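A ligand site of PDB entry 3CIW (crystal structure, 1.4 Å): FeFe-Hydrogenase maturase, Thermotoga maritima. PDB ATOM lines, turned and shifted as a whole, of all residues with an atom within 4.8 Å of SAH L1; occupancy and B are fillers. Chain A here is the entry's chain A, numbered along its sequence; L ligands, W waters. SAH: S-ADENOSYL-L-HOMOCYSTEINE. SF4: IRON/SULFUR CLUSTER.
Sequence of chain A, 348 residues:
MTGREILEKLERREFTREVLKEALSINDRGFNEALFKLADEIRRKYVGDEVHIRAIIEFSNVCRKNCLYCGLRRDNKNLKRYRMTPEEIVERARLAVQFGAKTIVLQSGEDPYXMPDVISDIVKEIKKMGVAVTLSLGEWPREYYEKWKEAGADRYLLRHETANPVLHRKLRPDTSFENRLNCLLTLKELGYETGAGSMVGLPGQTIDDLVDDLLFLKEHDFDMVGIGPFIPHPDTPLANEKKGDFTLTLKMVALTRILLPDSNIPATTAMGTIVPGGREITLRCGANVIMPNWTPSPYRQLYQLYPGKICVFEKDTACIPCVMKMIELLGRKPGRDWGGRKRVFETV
A nitrogen (N3) of SAH L1 lies close to the side-chain sulfur (SD) of Met 199, at 3.5 Å. CA of Cys 70 touches N7 of SAH L1, at 3.9 Å. Gln 107 touches SAH L1. Ser 136 touches SAH L1. Gly 138 touches SAH L1 (N to CA, 3.8 Å). O of Pro 229 touches C2 of SAH L1, 3.2 Å away. Phe 230 touches SAH L1 (CA to N1, 3.9 Å). Tyr 303 touches SAH L1. Leu 305 touches SAH L1 (CD1 to O4', 3.5 Å). CD2 of Tyr 306 touches C2 of SAH L1, 3.7 Å away.
An oxygen (O3') of SAH L1 is in hydrogen-bond range of the side-chain carboxylate of Glu 161 (2.5 Å). N of Ile 231 sits at hydrogen-bond distance from N1 of SAH L1 (3.0 Å). The backbone carbonyl oxygen of Ile 231 lies within hydrogen-bond range of a nitrogen (N6) of SAH L1, at 2.8 Å. O of Tyr 69 lies within hydrogen-bond range of N6 of SAH L1, at 2.9 Å. OXT of SAH L1 is in salt-bridge range of NH2 of Arg 180 (3.0 Å). NH1 of Arg 159 is in hydrogen-bond range of O2' of SAH L1 (3.0 Å). The backbone carbonyl oxygen (O) of Ser 108 sits close to a nitrogen (N) of SAH L1, 3.2 Å away. FE4 of SF4 L2 is bound by SG of Cys 70, 2.3 Å away.
An oxygen (O) of SAH L1 is bound to an iron atom (FE2) of SF4 L2, at 2.2 Å.
Water W1 bridges an oxygen (O3') of SAH L1 and the backbone NH (N) of Arg 159. Water W3 lies within hydrogen-bond range of an oxygen (OXT) of SAH L1 (2.8 Å), the side-chain hydroxyl of Ser 136 (3.0 Å), the backbone NH of Gly 138 (3.0 Å) and the backbone NH of Leu 137 (3.3 Å). Water W4 lies within hydrogen-bond range of OE2 of Glu 110 (2.7 Å), NH1 of Arg 180 (2.8 Å), NH2 of Arg 172 (3.3 Å) and S4 of SF4 L2 (3.3 Å). Water W5 lies within hydrogen-bond range of the side-chain carboxylate of Glu 161 (2.7 Å), the side-chain hydroxyl of Tyr 69 (2.8 Å), the guanidinium group of Arg 172 (3.1 Å) and a sulfur (S3) of SF4 L2 (3.2 Å).
The guanidinium group (NH2) of Arg 180 lies within salt-bridge range of the side-chain carboxylate (OE2) of Glu 161 (3.1 Å). The backbone carbonyl oxygen (O) of Glu 161 is in hydrogen-bond range of the backbone NH (N) of Met 199, 3.2 Å away. The side-chain hydroxyl of Tyr 69 is in hydrogen-bond range of the guanidinium group of Arg 172, 3.0 Å away. NE of Arg 180 is in hydrogen-bond range of O of Arg 159, 2.7 Å away. The backbone NH (N) of Ser 108 sits at hydrogen-bond distance from the backbone carbonyl oxygen (O) of Ser 136 (3.3 Å). The side-chain amide oxygen of Gln 107 sits at hydrogen-bond distance from the side-chain hydroxyl of Tyr 303. The side-chain hydroxyl (OG) of Ser 136 sits at hydrogen-bond distance from the side-chain amide nitrogen (NE2) of Gln 107 (3.1 Å). The backbone NH of Ala 270 is in hydrogen-bond range of the side-chain hydroxyl of Tyr 306, at 3.1 Å.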
ATOM      1  N   TYR A  69      20.895  -2.206 -31.034  1.00  0.00           N
ATOM      2  CA  TYR A  69      20.718  -0.970 -30.255  1.00  0.00           C
ATOM      3  C   TYR A  69      21.807  -0.728 -29.219  1.00  0.00           C
ATOM      4  O   TYR A  69      21.916   0.396 -28.712  1.00  0.00           O
ATOM      5  CB  TYR A  69      19.367  -0.984 -29.535  1.00  0.00           C
ATOM      6  CG  TYR A  69      19.045  -2.291 -28.863  1.00  0.00           C
ATOM      7  CD1 TYR A  69      19.593  -2.628 -27.621  1.00  0.00           C
ATOM      8  CD2 TYR A  69      18.212  -3.216 -29.471  1.00  0.00           C
ATOM      9  CE1 TYR A  69      19.292  -3.838 -27.012  1.00  0.00           C
ATOM     10  CE2 TYR A  69      17.916  -4.421 -28.874  1.00  0.00           C
ATOM     11  CZ  TYR A  69      18.446  -4.735 -27.646  1.00  0.00           C
ATOM     12  OH  TYR A  69      18.170  -5.949 -27.069  1.00  0.00           O
ATOM     13  N   CYS A  70      22.602  -1.753 -28.903  1.00  0.00           N
ATOM     14  CA  CYS A  70      23.407  -1.736 -27.686  1.00  0.00           C
ATOM     15  C   CYS A  70      24.870  -1.393 -27.915  1.00  0.00           C
ATOM     16  O   CYS A  70      25.530  -2.024 -28.745  1.00  0.00           O
ATOM     17  CB  CYS A  70      23.318  -3.092 -27.039  1.00  0.00           C
ATOM     18  SG  CYS A  70      24.153  -3.149 -25.421  1.00  0.00           S
ATOM     19  N   GLN A 107      24.919  -7.034 -13.047  1.00  0.00           N
ATOM     20  CA  GLN A 107      24.565  -6.946 -14.461  1.00  0.00           C
ATOM     21  C   GLN A 107      25.850  -6.969 -15.291  1.00  0.00           C
ATOM     22  O   GLN A 107      26.891  -6.429 -14.902  1.00  0.00           O
ATOM     23  CB  GLN A 107      23.790  -5.655 -14.765  1.00  0.00           C
ATOM     24  CG  GLN A 107      23.212  -5.644 -16.166  1.00  0.00           C
ATOM     25  CD  GLN A 107      22.386  -4.447 -16.466  1.00  0.00           C
ATOM     26  OE1 GLN A 107      22.900  -3.394 -16.810  1.00  0.00           O
ATOM     27  NE2 GLN A 107      21.068  -4.591 -16.354  1.00  0.00           N
ATOM     28  N   SER A 108      25.738  -7.569 -16.466  1.00  0.00           N
ATOM     29  CA  SER A 108      26.846  -7.598 -17.397  1.00  0.00           C
ATOM     30  C   SER A 108      26.348  -7.803 -18.803  1.00  0.00           C
ATOM     31  O   SER A 108      25.189  -8.155 -19.049  1.00  0.00           O
ATOM     32  CB  SER A 108      27.801  -8.732 -17.023  1.00  0.00           C
ATOM     33  OG  SER A 108      27.166 -10.010 -17.119  1.00  0.00           O
ATOM     34  N   GLY A 109      27.266  -7.610 -19.737  1.00  0.00           N
ATOM     35  CA  GLY A 109      27.077  -8.205 -21.066  1.00  0.00           C
ATOM     36  C   GLY A 109      27.028  -9.708 -20.923  1.00  0.00           C
ATOM     37  O   GLY A 109      27.363 -10.260 -19.865  1.00  0.00           O
ATOM     38  N   GLU A 110      26.655 -10.407 -21.993  1.00  0.00           N
ATOM     39  CA  GLU A 110      26.711 -11.856 -21.990  1.00  0.00           C
ATOM     40  C   GLU A 110      28.168 -12.279 -22.167  1.00  0.00           C
ATOM     41  O   GLU A 110      28.645 -12.576 -23.278  1.00  0.00           O
ATOM     42  CB  GLU A 110      25.823 -12.439 -23.080  1.00  0.00           C
ATOM     43  CG  GLU A 110      24.342 -12.256 -22.797  1.00  0.00           C
ATOM     44  CD  GLU A 110      23.451 -13.139 -23.659  1.00  0.00           C
ATOM     45  OE1 GLU A 110      24.000 -13.998 -24.372  1.00  0.00           O
ATOM     46  OE2 GLU A 110      22.217 -12.968 -23.610  1.00  0.00           O
ATOM     47  N   SER A 136      21.262  -9.978 -13.761  1.00  0.00           N
ATOM     48  CA  SER A 136      20.822  -9.496 -15.058  1.00  0.00           C
ATOM     49  C   SER A 136      21.955  -9.779 -16.034  1.00  0.00           C
ATOM     50  O   SER A 136      22.739  -8.896 -16.359  1.00  0.00           O
ATOM     51  CB  SER A 136      20.524  -8.008 -14.937  1.00  0.00           C
ATOM     52  OG  SER A 136      20.027  -7.462 -16.156  1.00  0.00           O
ATOM     53  N   LEU A 137      22.065 -11.043 -16.439  1.00  0.00           N
ATOM     54  CA  LEU A 137      23.201 -11.530 -17.207  1.00  0.00           C
ATOM     55  C   LEU A 137      22.844 -11.967 -18.609  1.00  0.00           C
ATOM     56  O   LEU A 137      23.713 -12.460 -19.332  1.00  0.00           O
ATOM     57  CB  LEU A 137      23.850 -12.695 -16.476  1.00  0.00           C
ATOM     58  CG  LEU A 137      24.110 -12.469 -14.993  1.00  0.00           C
ATOM     59  CD1 LEU A 137      24.747 -13.706 -14.332  1.00  0.00           C
ATOM     60  CD2 LEU A 137      24.969 -11.233 -14.756  1.00  0.00           C
ATOM     61  N   GLY A 138      21.586 -11.802 -19.012  1.00  0.00           N
ATOM     62  CA  GLY A 138      21.126 -12.211 -20.336  1.00  0.00           C
ATOM     63  C   GLY A 138      20.655 -13.647 -20.395  1.00  0.00           C
ATOM     64  O   GLY A 138      20.210 -14.228 -19.398  1.00  0.00           O
ATOM     65  N   LEU A 158      15.315  -9.762 -17.049  1.00  0.00           N
ATOM     66  CA  LEU A 158      15.523 -10.122 -18.449  1.00  0.00           C
ATOM     67  C   LEU A 158      14.442  -9.441 -19.276  1.00  0.00           C
ATOM     68  O   LEU A 158      13.375 -10.007 -19.547  1.00  0.00           O
ATOM     69  CB  LEU A 158      15.501 -11.634 -18.630  1.00  0.00           C
ATOM     70  CG  LEU A 158      16.035 -12.117 -19.975  1.00  0.00           C
ATOM     71  CD1 LEU A 158      17.564 -11.981 -20.079  1.00  0.00           C
ATOM     72  CD2 LEU A 158      15.633 -13.576 -20.206  1.00  0.00           C
ATOM     73  N   ARG A 159      14.670  -8.181 -19.595  1.00  0.00           N
ATOM     74  CA  ARG A 159      13.636  -7.433 -20.315  1.00  0.00           C
ATOM     75  C   ARG A 159      13.287  -8.176 -21.594  1.00  0.00           C
ATOM     76  O   ARG A 159      14.170  -8.682 -22.268  1.00  0.00           O
ATOM     77  CB  ARG A 159      14.140  -6.071 -20.665  1.00  0.00           C
ATOM     78  CG  ARG A 159      14.291  -5.181 -19.485  1.00  0.00           C
ATOM     79  CD  ARG A 159      14.648  -3.809 -19.973  1.00  0.00           C
ATOM     80  NE  ARG A 159      15.029  -2.914 -18.903  1.00  0.00           N
ATOM     81  CZ  ARG A 159      15.417  -1.663 -19.102  1.00  0.00           C
ATOM     82  NH1 ARG A 159      15.512  -1.181 -20.320  1.00  0.00           N
ATOM     83  NH2 ARG A 159      15.706  -0.900 -18.054  1.00  0.00           N
ATOM     84  N   GLU A 161      12.211  -6.765 -24.220  1.00  0.00           N
ATOM     85  CA  GLU A 161      12.725  -5.792 -25.195  1.00  0.00           C
ATOM     86  C   GLU A 161      11.642  -5.295 -26.139  1.00  0.00           C
ATOM     87  O   GLU A 161      11.406  -4.089 -26.251  1.00  0.00           O
ATOM     88  CB  GLU A 161      13.937  -6.326 -25.986  1.00  0.00           C
ATOM     89  CG  GLU A 161      15.053  -6.937 -25.138  1.00  0.00           C
ATOM     90  CD  GLU A 161      15.688  -6.001 -24.126  1.00  0.00           C
ATOM     91  OE1 GLU A 161      15.282  -4.836 -23.962  1.00  0.00           O
ATOM     92  OE2 GLU A 161      16.635  -6.494 -23.468  1.00  0.00           O
ATOM     93  N   ARG A 172      17.906  -8.233 -32.554  1.00  0.00           N
ATOM     94  CA  ARG A 172      18.656  -9.154 -31.705  1.00  0.00           C
ATOM     95  C   ARG A 172      18.957 -10.404 -32.546  1.00  0.00           C
ATOM     96  O   ARG A 172      18.350 -11.475 -32.348  1.00  0.00           O
ATOM     97  CB  ARG A 172      17.856  -9.450 -30.446  1.00  0.00           C
ATOM     98  CG  ARG A 172      17.348  -8.188 -29.759  1.00  0.00           C
ATOM     99  CD  ARG A 172      16.784  -8.393 -28.345  1.00  0.00           C
ATOM    100  NE  ARG A 172      17.865  -8.853 -27.493  1.00  0.00           N
ATOM    101  CZ  ARG A 172      17.985 -10.044 -26.942  1.00  0.00           C
ATOM    102  NH1 ARG A 172      17.019 -10.944 -27.014  1.00  0.00           N
ATOM    103  NH2 ARG A 172      19.087 -10.355 -26.280  1.00  0.00           N
ATOM    104  N   ARG A 180      13.664 -15.578 -25.778  1.00  0.00           N
ATOM    105  CA  ARG A 180      13.570 -14.635 -24.658  1.00  0.00           C
ATOM    106  C   ARG A 180      12.432 -15.014 -23.732  1.00  0.00           C
ATOM    107  O   ARG A 180      12.614 -15.051 -22.498  1.00  0.00           O
ATOM    108  CB  ARG A 180      13.375 -13.224 -25.199  1.00  0.00           C
ATOM    109  CG  ARG A 180      13.712 -12.100 -24.226  1.00  0.00           C
ATOM    110  CD  ARG A 180      15.201 -11.958 -24.063  1.00  0.00           C
ATOM    111  NE  ARG A 180      15.574 -10.747 -23.342  1.00  0.00           N
ATOM    112  CZ  ARG A 180      16.828 -10.416 -23.050  1.00  0.00           C
ATOM    113  NH1 ARG A 180      17.837 -11.189 -23.410  1.00  0.00           N
ATOM    114  NH2 ARG A 180      17.099  -9.309 -22.343  1.00  0.00           N
ATOM    115  N   MET A 199      11.907  -1.573 -24.356  1.00  0.00           N
ATOM    116  CA  MET A 199      12.293  -0.241 -24.768  1.00  0.00           C
ATOM    117  C   MET A 199      11.142   0.370 -25.548  1.00  0.00           C
ATOM    118  O   MET A 199      10.337  -0.345 -26.159  1.00  0.00           O
ATOM    119  CB  MET A 199      13.586  -0.251 -25.581  1.00  0.00           C
ATOM    120  CG  MET A 199      14.852  -0.511 -24.745  1.00  0.00           C
ATOM    121  SD  MET A 199      16.287  -0.758 -25.787  1.00  0.00           S
ATOM    122  CE  MET A 199      15.972  -2.374 -26.441  1.00  0.00           C
ATOM    123  N   PRO A 229      13.299   4.485 -22.561  1.00  0.00           N
ATOM    124  CA  PRO A 229      13.320   4.887 -23.954  1.00  0.00           C
ATOM    125  C   PRO A 229      14.540   4.322 -24.647  1.00  0.00           C
ATOM    126  O   PRO A 229      15.583   4.224 -24.046  1.00  0.00           O
ATOM    127  CB  PRO A 229      13.466   6.409 -23.858  1.00  0.00           C
ATOM    128  CG  PRO A 229      14.259   6.637 -22.610  1.00  0.00           C
ATOM    129  CD  PRO A 229      13.757   5.551 -21.664  1.00  0.00           C
ATOM    130  N   PHE A 230      14.382   4.012 -25.918  1.00  0.00           N
ATOM    131  CA  PHE A 230      15.530   3.741 -26.751  1.00  0.00           C
ATOM    132  C   PHE A 230      16.405   5.002 -26.894  1.00  0.00           C
ATOM    133  O   PHE A 230      15.887   6.066 -27.243  1.00  0.00           O
ATOM    134  CB  PHE A 230      15.057   3.282 -28.127  1.00  0.00           C
ATOM    135  CG  PHE A 230      16.144   3.306 -29.175  1.00  0.00           C
ATOM    136  CD1 PHE A 230      17.246   2.489 -29.054  1.00  0.00           C
ATOM    137  CD2 PHE A 230      16.051   4.163 -30.253  1.00  0.00           C
ATOM    138  CE1 PHE A 230      18.259   2.514 -29.999  1.00  0.00           C
ATOM    139  CE2 PHE A 230      17.062   4.189 -31.216  1.00  0.00           C
ATOM    140  CZ  PHE A 230      18.166   3.371 -31.077  1.00  0.00           C
ATOM    141  N   ILE A 231      17.700   4.857 -26.640  1.00  0.00           N
ATOM    142  CA  ILE A 231      18.657   5.940 -26.788  1.00  0.00           C
ATOM    143  C   ILE A 231      19.750   5.512 -27.787  1.00  0.00           C
ATOM    144  O   ILE A 231      20.533   4.598 -27.501  1.00  0.00           O
ATOM    145  CB  ILE A 231      19.282   6.321 -25.432  1.00  0.00           C
ATOM    146  CG1 ILE A 231      18.213   6.748 -24.424  1.00  0.00           C
ATOM    147  CG2 ILE A 231      20.295   7.450 -25.603  1.00  0.00           C
ATOM    148  CD1 ILE A 231      18.700   6.972 -23.022  1.00  0.00           C
ATOM    149  N   ALA A 270      17.806   5.293 -17.943  1.00  0.00           N
ATOM    150  CA  ALA A 270      17.561   5.842 -19.280  1.00  0.00           C
ATOM    151  C   ALA A 270      16.541   6.987 -19.220  1.00  0.00           C
ATOM    152  O   ALA A 270      16.691   7.959 -19.941  1.00  0.00           O
ATOM    153  CB  ALA A 270      17.099   4.746 -20.242  1.00  0.00           C
ATOM    154  N   TYR A 303      30.757   1.200 -19.305  1.00  0.00           N
ATOM    155  CA  TYR A 303      29.543   0.422 -19.442  1.00  0.00           C
ATOM    156  C   TYR A 303      28.507   1.279 -20.106  1.00  0.00           C
ATOM    157  O   TYR A 303      27.652   1.856 -19.463  1.00  0.00           O
ATOM    158  CB  TYR A 303      29.069  -0.073 -18.096  1.00  0.00           C
ATOM    159  CG  TYR A 303      28.044  -1.178 -18.185  1.00  0.00           C
ATOM    160  CD1 TYR A 303      28.418  -2.507 -18.386  1.00  0.00           C
ATOM    161  CD2 TYR A 303      26.686  -0.895 -18.071  1.00  0.00           C
ATOM    162  CE1 TYR A 303      27.476  -3.516 -18.447  1.00  0.00           C
ATOM    163  CE2 TYR A 303      25.751  -1.899 -18.128  1.00  0.00           C
ATOM    164  CZ  TYR A 303      26.143  -3.197 -18.324  1.00  0.00           C
ATOM    165  OH  TYR A 303      25.186  -4.176 -18.353  1.00  0.00           O
ATOM    166  N   LEU A 305      25.762   1.109 -22.513  1.00  0.00           N
ATOM    167  CA  LEU A 305      24.659   0.519 -23.298  1.00  0.00           C
ATOM    168  C   LEU A 305      24.138   1.597 -24.263  1.00  0.00           C
ATOM    169  O   LEU A 305      23.879   1.339 -25.421  1.00  0.00           O
ATOM    170  CB  LEU A 305      23.539   0.027 -22.366  1.00  0.00           C
ATOM    171  CG  LEU A 305      23.887  -1.010 -21.296  1.00  0.00           C
ATOM    172  CD1 LEU A 305      22.712  -1.183 -20.318  1.00  0.00           C
ATOM    173  CD2 LEU A 305      24.235  -2.329 -21.941  1.00  0.00           C
ATOM    174  N   TYR A 306      23.989   2.796 -23.722  1.00  0.00           N
ATOM    175  CA  TYR A 306      23.638   3.993 -24.448  1.00  0.00           C
ATOM    176  C   TYR A 306      24.514   5.127 -23.944  1.00  0.00           C
ATOM    177  O   TYR A 306      25.044   5.070 -22.824  1.00  0.00           O
ATOM    178  CB  TYR A 306      22.149   4.323 -24.235  1.00  0.00           C
ATOM    179  CG  TYR A 306      21.706   4.298 -22.790  1.00  0.00           C
ATOM    180  CD1 TYR A 306      21.890   5.413 -21.967  1.00  0.00           C
ATOM    181  CD2 TYR A 306      21.127   3.168 -22.243  1.00  0.00           C
ATOM    182  CE1 TYR A 306      21.509   5.398 -20.657  1.00  0.00           C
ATOM    183  CE2 TYR A 306      20.736   3.143 -20.909  1.00  0.00           C
ATOM    184  CZ  TYR A 306      20.930   4.261 -20.122  1.00  0.00           C
ATOM    185  OH  TYR A 306      20.547   4.263 -18.806  1.00  0.00           O
HETATM  186  N   SAH L   1      23.062  -8.321 -21.398  1.00  0.00           N
HETATM  187  CA  SAH L   1      21.899  -8.324 -20.479  1.00  0.00           C
HETATM  188  CB  SAH L   1      21.960  -7.164 -19.489  1.00  0.00           C
HETATM  189  CG  SAH L   1      22.526  -5.845 -19.981  1.00  0.00           C
HETATM  190  SD  SAH L   1      21.497  -4.986 -21.188  1.00  0.00           S
HETATM  191  C   SAH L   1      20.627  -8.320 -21.317  1.00  0.00           C
HETATM  192  O   SAH L   1      20.710  -8.062 -22.541  1.00  0.00           O
HETATM  193  OXT SAH L   1      19.541  -8.566 -20.765  1.00  0.00           O
HETATM  194  C5' SAH L   1      20.204  -4.322 -20.074  1.00  0.00           C
HETATM  195  C4' SAH L   1      19.099  -3.515 -20.772  1.00  0.00           C
HETATM  196  O4' SAH L   1      19.549  -2.272 -21.305  1.00  0.00           O
HETATM  197  C3' SAH L   1      18.472  -4.213 -21.980  1.00  0.00           C
HETATM  198  O3' SAH L   1      17.521  -5.148 -21.549  1.00  0.00           O
HETATM  199  C2' SAH L   1      17.892  -3.063 -22.814  1.00  0.00           C
HETATM  200  O2' SAH L   1      16.499  -2.871 -22.623  1.00  0.00           O
HETATM  201  C1' SAH L   1      18.662  -1.816 -22.286  1.00  0.00           C
HETATM  202  N9  SAH L   1      19.355  -1.123 -23.362  1.00  0.00           N
HETATM  203  C8  SAH L   1      20.367  -1.614 -24.150  1.00  0.00           C
HETATM  204  N7  SAH L   1      20.706  -0.692 -25.088  1.00  0.00           N
HETATM  205  C5  SAH L   1      19.886   0.381 -24.945  1.00  0.00           C
HETATM  206  C6  SAH L   1      19.795   1.597 -25.581  1.00  0.00           C
HETATM  207  N6  SAH L   1      20.551   1.914 -26.642  1.00  0.00           N
HETATM  208  N1  SAH L   1      18.843   2.469 -25.160  1.00  0.00           N
HETATM  209  C2  SAH L   1      18.038   2.210 -24.085  1.00  0.00           C
HETATM  210  N3  SAH L   1      18.156   1.030 -23.423  1.00  0.00           N
HETATM  211  C4  SAH L   1      19.055   0.126 -23.837  1.00  0.00           C
HETATM  212 FE1  SF4 L   2      22.464  -7.408 -26.218  1.00  0.00          FE
HETATM  213 FE2  SF4 L   2      22.629  -7.311 -23.401  1.00  0.00          FE
HETATM  214 FE3  SF4 L   2      24.897  -7.806 -25.055  1.00  0.00          FE
HETATM  215 FE4  SF4 L   2      23.814  -5.363 -25.061  1.00  0.00          FE
HETATM  216  S1  SF4 L   2      24.791  -6.344 -23.294  1.00  0.00           S
HETATM  217  S2  SF4 L   2      24.510  -6.546 -26.910  1.00  0.00           S
HETATM  218  S3  SF4 L   2      21.566  -5.816 -24.792  1.00  0.00           S
HETATM  219  S4  SF4 L   2      23.010  -9.130 -24.852  1.00  0.00           S
HETATM  220  O   HOH W   1      17.461  -7.067 -19.643  1.00  0.00           O
HETATM  221  O   HOH W   2      19.447  -0.938 -18.880  1.00  0.00           O
HETATM  222  O   HOH W   3      19.675  -9.627 -18.139  1.00  0.00           O
HETATM  223  O   HOH W   4      20.611 -10.867 -23.406  1.00  0.00           O
HETATM  224  O   HOH W   5      18.792  -7.481 -24.834  1.00  0.00           O
